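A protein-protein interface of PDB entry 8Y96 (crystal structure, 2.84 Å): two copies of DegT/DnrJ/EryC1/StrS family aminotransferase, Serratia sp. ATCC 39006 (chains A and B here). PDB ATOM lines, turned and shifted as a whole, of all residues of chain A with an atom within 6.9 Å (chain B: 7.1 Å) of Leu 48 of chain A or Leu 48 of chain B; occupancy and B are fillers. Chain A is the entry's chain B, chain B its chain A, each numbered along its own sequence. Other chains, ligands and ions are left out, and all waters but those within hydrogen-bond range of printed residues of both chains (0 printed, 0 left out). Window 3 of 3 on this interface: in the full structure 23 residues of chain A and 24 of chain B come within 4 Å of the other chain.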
ATOM      1  N   ILE A  43     -27.239   3.811  -2.756  1.00  0.00           N
ATOM      2  CA  ILE A  43     -27.070   2.847  -3.827  1.00  0.00           C
ATOM      3  C   ILE A  43     -28.305   1.953  -3.863  1.00  0.00           C
ATOM      4  O   ILE A  43     -28.545   1.187  -2.934  1.00  0.00           O
ATOM      5  CB  ILE A  43     -25.760   2.056  -3.658  1.00  0.00           C
ATOM      6  CG1 ILE A  43     -24.557   3.003  -3.687  1.00  0.00           C
ATOM      7  CG2 ILE A  43     -25.642   0.959  -4.719  1.00  0.00           C
ATOM      8  CD1 ILE A  43     -23.205   2.324  -3.591  1.00  0.00           C
ATOM      9  N   ALA A  44     -29.081   2.082  -4.946  1.00  0.00           N
ATOM     10  CA  ALA A  44     -30.318   1.339  -5.125  1.00  0.00           C
ATOM     11  C   ALA A  44     -30.166   0.378  -6.297  1.00  0.00           C
ATOM     12  O   ALA A  44     -29.218   0.486  -7.070  1.00  0.00           O
ATOM     13  CB  ALA A  44     -31.465   2.295  -5.347  1.00  0.00           C
ATOM     14  N   LYS A  45     -31.127  -0.547  -6.412  1.00  0.00           N
ATOM     15  CA  LYS A  45     -31.152  -1.546  -7.470  1.00  0.00           C
ATOM     16  C   LYS A  45     -30.947  -0.894  -8.836  1.00  0.00           C
ATOM     17  O   LYS A  45     -30.258  -1.446  -9.692  1.00  0.00           O
ATOM     18  CB  LYS A  45     -32.471  -2.324  -7.439  1.00  0.00           C
ATOM     19  CG  LYS A  45     -33.762  -1.511  -7.541  1.00  0.00           C
ATOM     20  CD  LYS A  45     -34.992  -2.379  -7.300  1.00  0.00           C
ATOM     21  CE  LYS A  45     -36.246  -1.611  -7.048  1.00  0.00           C
ATOM     22  NZ  LYS A  45     -36.808  -1.036  -8.270  1.00  0.00           N
ATOM     23  N   GLU A  46     -31.540   0.289  -9.022  1.00  0.00           N
ATOM     24  CA  GLU A  46     -31.443   1.025 -10.272  1.00  0.00           C
ATOM     25  C   GLU A  46     -29.981   1.168 -10.688  1.00  0.00           C
ATOM     26  O   GLU A  46     -29.652   0.998 -11.859  1.00  0.00           O
ATOM     27  CB  GLU A  46     -32.099   2.404 -10.141  1.00  0.00           C
ATOM     28  CG  GLU A  46     -33.625   2.365 -10.084  1.00  0.00           C
ATOM     29  CD  GLU A  46     -34.249   1.935  -8.766  1.00  0.00           C
ATOM     30  OE1 GLU A  46     -33.558   1.927  -7.729  1.00  0.00           O
ATOM     31  OE2 GLU A  46     -35.448   1.587  -8.789  1.00  0.00           O
ATOM     32  N   ASP A  47     -29.114   1.476  -9.716  1.00  0.00           N
ATOM     33  CA  ASP A  47     -27.718   1.777  -9.985  1.00  0.00           C
ATOM     34  C   ASP A  47     -26.985   0.518 -10.451  1.00  0.00           C
ATOM     35  O   ASP A  47     -26.106   0.603 -11.308  1.00  0.00           O
ATOM     36  CB  ASP A  47     -27.054   2.410  -8.773  1.00  0.00           C
ATOM     37  CG  ASP A  47     -27.761   3.625  -8.190  1.00  0.00           C
ATOM     38  OD1 ASP A  47     -28.067   4.564  -8.957  1.00  0.00           O
ATOM     39  OD2 ASP A  47     -27.994   3.625  -6.965  1.00  0.00           O
ATOM     40  N   LEU A  48     -27.344  -0.638  -9.871  1.00  0.00           N
ATOM     41  CA  LEU A  48     -26.775  -1.919 -10.261  1.00  0.00           C
ATOM     42  C   LEU A  48     -27.230  -2.272 -11.673  1.00  0.00           C
ATOM     43  O   LEU A  48     -26.447  -2.770 -12.477  1.00  0.00           O
ATOM     44  CB  LEU A  48     -27.169  -3.033  -9.292  1.00  0.00           C
ATOM     45  CG  LEU A  48     -26.282  -3.206  -8.057  1.00  0.00           C
ATOM     46  CD1 LEU A  48     -26.413  -2.032  -7.101  1.00  0.00           C
ATOM     47  CD2 LEU A  48     -26.622  -4.512  -7.360  1.00  0.00           C
ATOM     48  N   PHE A  49     -28.516  -2.053 -11.953  1.00  0.00           N
ATOM     49  CA  PHE A  49     -29.062  -2.395 -13.253  1.00  0.00           C
ATOM     50  C   PHE A  49     -28.453  -1.481 -14.315  1.00  0.00           C
ATOM     51  O   PHE A  49     -28.150  -1.933 -15.417  1.00  0.00           O
ATOM     52  CB  PHE A  49     -30.589  -2.301 -13.211  1.00  0.00           C
ATOM     53  CG  PHE A  49     -31.254  -2.650 -14.533  1.00  0.00           C
ATOM     54  CD1 PHE A  49     -30.910  -3.805 -15.221  1.00  0.00           C
ATOM     55  CD2 PHE A  49     -32.196  -1.803 -15.096  1.00  0.00           C
ATOM     56  CE1 PHE A  49     -31.516  -4.116 -16.426  1.00  0.00           C
ATOM     57  CE2 PHE A  49     -32.795  -2.115 -16.302  1.00  0.00           C
ATOM     58  CZ  PHE A  49     -32.452  -3.269 -16.966  1.00  0.00           C
ATOM     59  N   GLN A  50     -28.248  -0.205 -13.957  1.00  0.00           N
ATOM     60  CA  GLN A  50     -27.671   0.782 -14.860  1.00  0.00           C
ATOM     61  C   GLN A  50     -26.251   0.394 -15.267  1.00  0.00           C
ATOM     62  O   GLN A  50     -25.802   0.762 -16.350  1.00  0.00           O
ATOM     63  CB  GLN A  50     -27.657   2.159 -14.198  1.00  0.00           C
ATOM     64  CG  GLN A  50     -27.123   3.286 -15.078  1.00  0.00           C
ATOM     65  CD  GLN A  50     -27.957   3.528 -16.316  1.00  0.00           C
ATOM     66  OE1 GLN A  50     -29.110   3.963 -16.232  1.00  0.00           O
ATOM     67  NE2 GLN A  50     -27.388   3.258 -17.482  1.00  0.00           N
ATOM     68  N   MET A  51     -25.536  -0.323 -14.392  1.00  0.00           N
ATOM     69  CA  MET A  51     -24.193  -0.787 -14.697  1.00  0.00           C
ATOM     70  C   MET A  51     -24.245  -1.908 -15.729  1.00  0.00           C
ATOM     71  O   MET A  51     -23.312  -2.060 -16.513  1.00  0.00           O
ATOM     72  CB  MET A  51     -23.468  -1.284 -13.443  1.00  0.00           C
ATOM     73  CG  MET A  51     -23.068  -0.178 -12.498  1.00  0.00           C
ATOM     74  SD  MET A  51     -21.820   0.912 -13.212  1.00  0.00           S
ATOM     75  CE  MET A  51     -21.781   2.077 -11.845  1.00  0.00           C
ATOM     76  N   MET A  52     -25.336  -2.684 -15.719  1.00  0.00           N
ATOM     77  CA  MET A  52     -25.491  -3.790 -16.650  1.00  0.00           C
ATOM     78  C   MET A  52     -25.958  -3.269 -18.008  1.00  0.00           C
ATOM     79  O   MET A  52     -25.765  -3.944 -19.015  1.00  0.00           O
ATOM     80  CB  MET A  52     -26.463  -4.842 -16.102  1.00  0.00           C
ATOM     81  CG  MET A  52     -25.992  -5.471 -14.805  1.00  0.00           C
ATOM     82  SD  MET A  52     -27.160  -6.658 -14.112  1.00  0.00           S
ATOM     83  CE  MET A  52     -26.843  -8.017 -15.244  1.00  0.00           C
ATOM     84  N   ILE A  53     -26.564  -2.072 -18.037  1.00  0.00           N
ATOM     85  CA  ILE A  53     -26.935  -1.430 -19.290  1.00  0.00           C
ATOM     86  C   ILE A  53     -25.691  -0.807 -19.925  1.00  0.00           C
ATOM     87  O   ILE A  53     -25.441  -0.999 -21.112  1.00  0.00           O
ATOM     88  CB  ILE A  53     -28.053  -0.387 -19.085  1.00  0.00           C
ATOM     89  CG1 ILE A  53     -29.384  -1.046 -18.724  1.00  0.00           C
ATOM     90  CG2 ILE A  53     -28.200   0.515 -20.312  1.00  0.00           C
ATOM     91  CD1 ILE A  53     -30.434  -0.081 -18.196  1.00  0.00           C
ATOM     92  N   PHE A 253     -22.952   5.404 -12.936  1.00  0.00           N
ATOM     93  CA  PHE A 253     -23.540   5.634 -11.628  1.00  0.00           C
ATOM     94  C   PHE A 253     -24.249   6.989 -11.622  1.00  0.00           C
ATOM     95  O   PHE A 253     -25.323   7.125 -11.042  1.00  0.00           O
ATOM     96  CB  PHE A 253     -22.439   5.505 -10.571  1.00  0.00           C
ATOM     97  CG  PHE A 253     -22.955   5.443  -9.140  1.00  0.00           C
ATOM     98  CD1 PHE A 253     -23.521   4.277  -8.640  1.00  0.00           C
ATOM     99  CD2 PHE A 253     -22.878   6.551  -8.306  1.00  0.00           C
ATOM    100  CE1 PHE A 253     -23.999   4.225  -7.342  1.00  0.00           C
ATOM    101  CE2 PHE A 253     -23.358   6.495  -7.009  1.00  0.00           C
ATOM    102  CZ  PHE A 253     -23.914   5.332  -6.530  1.00  0.00           C
ATOM    103  N   SER A 256     -27.921   6.857 -13.522  1.00  0.00           N
ATOM    104  CA  SER A 256     -28.986   6.347 -12.675  1.00  0.00           C
ATOM    105  C   SER A 256     -29.276   7.327 -11.540  1.00  0.00           C
ATOM    106  O   SER A 256     -30.431   7.701 -11.344  1.00  0.00           O
ATOM    107  CB  SER A 256     -28.678   4.964 -12.152  1.00  0.00           C
ATOM    108  OG  SER A 256     -27.313   4.825 -11.788  1.00  0.00           O
ATOM    109  N   ILE B  43     -37.322  -4.311  -2.817  1.00  0.00           N
ATOM    110  CA  ILE B  43     -36.245  -4.851  -3.633  1.00  0.00           C
ATOM    111  C   ILE B  43     -35.056  -3.897  -3.558  1.00  0.00           C
ATOM    112  O   ILE B  43     -35.098  -2.794  -4.095  1.00  0.00           O
ATOM    113  CB  ILE B  43     -36.705  -5.101  -5.082  1.00  0.00           C
ATOM    114  CG1 ILE B  43     -37.954  -5.979  -5.129  1.00  0.00           C
ATOM    115  CG2 ILE B  43     -35.578  -5.703  -5.921  1.00  0.00           C
ATOM    116  CD1 ILE B  43     -38.668  -5.964  -6.468  1.00  0.00           C
ATOM    117  N   ALA B  44     -34.000  -4.336  -2.870  1.00  0.00           N
ATOM    118  CA  ALA B  44     -32.804  -3.534  -2.698  1.00  0.00           C
ATOM    119  C   ALA B  44     -31.667  -4.136  -3.518  1.00  0.00           C
ATOM    120  O   ALA B  44     -31.826  -5.200  -4.112  1.00  0.00           O
ATOM    121  CB  ALA B  44     -32.457  -3.456  -1.228  1.00  0.00           C
ATOM    122  N   LYS B  45     -30.522  -3.442  -3.521  1.00  0.00           N
ATOM    123  CA  LYS B  45     -29.348  -3.833  -4.292  1.00  0.00           C
ATOM    124  C   LYS B  45     -28.880  -5.238  -3.916  1.00  0.00           C
ATOM    125  O   LYS B  45     -28.331  -5.948  -4.753  1.00  0.00           O
ATOM    126  CB  LYS B  45     -28.200  -2.838  -4.071  1.00  0.00           C
ATOM    127  CG  LYS B  45     -27.674  -2.764  -2.642  1.00  0.00           C
ATOM    128  CD  LYS B  45     -26.625  -1.685  -2.416  1.00  0.00           C
ATOM    129  CE  LYS B  45     -26.206  -1.613  -0.978  1.00  0.00           C
ATOM    130  NZ  LYS B  45     -24.982  -0.825  -0.822  1.00  0.00           N
ATOM    131  N   GLU B  46     -29.093  -5.621  -2.650  1.00  0.00           N
ATOM    132  CA  GLU B  46     -28.661  -6.912  -2.139  1.00  0.00           C
ATOM    133  C   GLU B  46     -29.375  -8.047  -2.873  1.00  0.00           C
ATOM    134  O   GLU B  46     -28.813  -9.121  -3.042  1.00  0.00           O
ATOM    135  CB  GLU B  46     -28.908  -7.016  -0.631  1.00  0.00           C
ATOM    136  CG  GLU B  46     -28.002  -6.120   0.213  1.00  0.00           C
ATOM    137  CD  GLU B  46     -28.346  -4.640   0.257  1.00  0.00           C
ATOM    138  OE1 GLU B  46     -29.429  -4.254  -0.222  1.00  0.00           O
ATOM    139  OE2 GLU B  46     -27.516  -3.859   0.771  1.00  0.00           O
ATOM    140  N   ASP B  47     -30.614  -7.800  -3.308  1.00  0.00           N
ATOM    141  CA  ASP B  47     -31.423  -8.824  -3.948  1.00  0.00           C
ATOM    142  C   ASP B  47     -30.927  -9.072  -5.371  1.00  0.00           C
ATOM    143  O   ASP B  47     -30.959 -10.204  -5.844  1.00  0.00           O
ATOM    144  CB  ASP B  47     -32.897  -8.460  -3.889  1.00  0.00           C
ATOM    145  CG  ASP B  47     -33.412  -8.186  -2.484  1.00  0.00           C
ATOM    146  OD1 ASP B  47     -33.201  -9.052  -1.608  1.00  0.00           O
ATOM    147  OD2 ASP B  47     -34.004  -7.106  -2.274  1.00  0.00           O
ATOM    148  N   LEU B  48     -30.480  -8.012  -6.052  1.00  0.00           N
ATOM    149  CA  LEU B  48     -29.959  -8.151  -7.401  1.00  0.00           C
ATOM    150  C   LEU B  48     -28.643  -8.924  -7.365  1.00  0.00           C
ATOM    151  O   LEU B  48     -28.408  -9.800  -8.198  1.00  0.00           O
ATOM    152  CB  LEU B  48     -29.786  -6.789  -8.072  1.00  0.00           C
ATOM    153  CG  LEU B  48     -30.995  -6.290  -8.868  1.00  0.00           C
ATOM    154  CD1 LEU B  48     -32.163  -5.942  -7.957  1.00  0.00           C
ATOM    155  CD2 LEU B  48     -30.604  -5.108  -9.734  1.00  0.00           C
ATOM    156  N   PHE B  49     -27.788  -8.588  -6.395  1.00  0.00           N
ATOM    157  CA  PHE B  49     -26.497  -9.239  -6.264  1.00  0.00           C
ATOM    158  C   PHE B  49     -26.715 -10.723  -5.980  1.00  0.00           C
ATOM    159  O   PHE B  49     -25.964 -11.564  -6.471  1.00  0.00           O
ATOM    160  CB  PHE B  49     -25.658  -8.573  -5.170  1.00  0.00           C
ATOM    161  CG  PHE B  49     -24.224  -9.080  -5.104  1.00  0.00           C
ATOM    162  CD1 PHE B  49     -23.470  -9.256  -6.262  1.00  0.00           C
ATOM    163  CD2 PHE B  49     -23.638  -9.401  -3.884  1.00  0.00           C
ATOM    164  CE1 PHE B  49     -22.167  -9.727  -6.197  1.00  0.00           C
ATOM    165  CE2 PHE B  49     -22.334  -9.873  -3.826  1.00  0.00           C
ATOM    166  CZ  PHE B  49     -21.604 -10.037  -4.981  1.00  0.00           C
ATOM    167  N   GLN B  50     -27.765 -11.027  -5.205  1.00  0.00           N
ATOM    168  CA  GLN B  50     -28.073 -12.390  -4.807  1.00  0.00           C
ATOM    169  C   GLN B  50     -28.346 -13.246  -6.041  1.00  0.00           C
ATOM    170  O   GLN B  50     -27.918 -14.396  -6.095  1.00  0.00           O
ATOM    171  CB  GLN B  50     -29.249 -12.401  -3.831  1.00  0.00           C
ATOM    172  CG  GLN B  50     -29.514 -13.750  -3.166  1.00  0.00           C
ATOM    173  CD  GLN B  50     -28.379 -14.240  -2.289  1.00  0.00           C
ATOM    174  OE1 GLN B  50     -27.853 -13.509  -1.442  1.00  0.00           O
ATOM    175  NE2 GLN B  50     -27.982 -15.486  -2.485  1.00  0.00           N
ATOM    176  N   MET B  51     -29.035 -12.679  -7.036  1.00  0.00           N
ATOM    177  CA  MET B  51     -29.314 -13.397  -8.271  1.00  0.00           C
ATOM    178  C   MET B  51     -28.015 -13.753  -8.991  1.00  0.00           C
ATOM    179  O   MET B  51     -27.922 -14.811  -9.599  1.00  0.00           O
ATOM    180  CB  MET B  51     -30.203 -12.578  -9.211  1.00  0.00           C
ATOM    181  CG  MET B  51     -31.585 -12.321  -8.655  1.00  0.00           C
ATOM    182  SD  MET B  51     -32.408 -13.852  -8.175  1.00  0.00           S
ATOM    183  CE  MET B  51     -33.778 -13.180  -7.224  1.00  0.00           C
ATOM    184  N   MET B  52     -27.018 -12.868  -8.916  1.00  0.00           N
ATOM    185  CA  MET B  52     -25.755 -13.077  -9.608  1.00  0.00           C
ATOM    186  C   MET B  52     -24.894 -14.079  -8.839  1.00  0.00           C
ATOM    187  O   MET B  52     -24.007 -14.701  -9.418  1.00  0.00           O
ATOM    188  CB  MET B  52     -25.024 -11.746  -9.804  1.00  0.00           C
ATOM    189  CG  MET B  52     -25.856 -10.732 -10.563  1.00  0.00           C
ATOM    190  SD  MET B  52     -25.040  -9.137 -10.742  1.00  0.00           S
ATOM    191  CE  MET B  52     -23.880  -9.524 -12.059  1.00  0.00           C
ATOM    192  N   ILE B  53     -25.160 -14.237  -7.538  1.00  0.00           N
ATOM    193  CA  ILE B  53     -24.519 -15.279  -6.756  1.00  0.00           C
ATOM    194  C   ILE B  53     -25.175 -16.612  -7.102  1.00  0.00           C
ATOM    195  O   ILE B  53     -24.488 -17.556  -7.483  1.00  0.00           O
ATOM    196  CB  ILE B  53     -24.584 -14.965  -5.247  1.00  0.00           C
ATOM    197  CG1 ILE B  53     -23.651 -13.802  -4.890  1.00  0.00           C
ATOM    198  CG2 ILE B  53     -24.281 -16.204  -4.403  1.00  0.00           C
ATOM    199  CD1 ILE B  53     -23.811 -13.273  -3.475  1.00  0.00           C
ATOM    200  N   PHE B 253     -34.282 -14.963  -4.090  1.00  0.00           N
ATOM    201  CA  PHE B 253     -34.846 -13.736  -3.553  1.00  0.00           C
ATOM    202  C   PHE B 253     -35.136 -13.930  -2.065  1.00  0.00           C
ATOM    203  O   PHE B 253     -34.909 -13.022  -1.269  1.00  0.00           O
ATOM    204  CB  PHE B 253     -36.064 -13.367  -4.403  1.00  0.00           C
ATOM    205  CG  PHE B 253     -36.637 -11.988  -4.115  1.00  0.00           C
ATOM    206  CD1 PHE B 253     -36.058 -10.849  -4.663  1.00  0.00           C
ATOM    207  CD2 PHE B 253     -37.760 -11.839  -3.309  1.00  0.00           C
ATOM    208  CE1 PHE B 253     -36.586  -9.594  -4.399  1.00  0.00           C
ATOM    209  CE2 PHE B 253     -38.284 -10.583  -3.048  1.00  0.00           C
ATOM    210  CZ  PHE B 253     -37.696  -9.464  -3.593  1.00  0.00           C
ATOM    211  N   SER B 256     -31.773 -13.489   0.197  1.00  0.00           N
ATOM    212  CA  SER B 256     -31.378 -12.112   0.439  1.00  0.00           C
ATOM    213  C   SER B 256     -32.409 -11.392   1.305  1.00  0.00           C
ATOM    214  O   SER B 256     -32.048 -10.591   2.164  1.00  0.00           O
ATOM    215  CB  SER B 256     -31.166 -11.389  -0.860  1.00  0.00           C
ATOM    216  OG  SER B 256     -32.288 -11.547  -1.716  1.00  0.00           O
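The side-chain amino group (NZ) of Lys 45 of chain A lies within salt-bridge range of the side-chain carboxylate (OE2) of Glu 46 of chain A, at 3.0 Å.
Lys 45 of chain B touches Ile 43 of chain A (CD to O, 3.5 Å).
Ile 43 of chain B touches Lys 45 of chain A (O to CD, 3.2 Å).
Leu 48 of chain B touches Lys 45 of chain A (CD1 to CB, 3.7 Å).
CD2 of Leu 48 of chain A touches O of Lys 45 of chain B (3.4 Å).
Leu 48 of chain A touches Leu 48 of chain B (CD2 to CB, 3.96 Å).
Leu 48 of chain B touches just these residues of chain A: Lys 45 and Leu 48.
Printed residues of chain B within 4 Å of Lys 45 of chain A: Ile 43 (3.2 Å) and Leu 48 (3.7 Å).
Printed residues of chain A within 4 Å of Lys 45 of chain B: Ile 43 and Leu 48.
Of the printed residues of chain A, Ile 43 of chain B touches Lys 45.
Phe 49 of chain B touches none of the printed residues of chain A.
Glu 46 of chain A touches none of the printed residues of chain B.
The nearest residue of chain A that does not touch Leu 48 of chain B is Phe 49 of chain A (4.3 Å).
The nearest printed residue of chain A that does not touch Ile 43 of chain B is Glu 46 of chain A (6.2 Å).
Of the 13 printed residues of chain B, 3 touch a printed residue of chain A.
Printed residues of chain B that touch a printed residue of chain A: Ile 43, Lys 45 and Leu 48.
Hydrophobic or aromatic side chains of chain B that line the printed part of chain A: Ile 43 and Leu 48.
Printed residues of chain A that touch a printed residue of chain B: Ile 43, Lys 45 and Leu 48.
Among the printed residues, 5 pairs touch across the chains.
Ile 43 of chain A touches Lys 45 of chain B, and with the chains exchanged Lys 45 of chain A touches Ile 43 of chain B.
Lys 45 of chain A touches Leu 48 of chain B, and with the chains exchanged Leu 48 of chain A touches Lys 45 of chain B.
Leu 48 of chain A touches its own counterpart, Leu 48 of chain B.
13 positions are printed for both chains.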
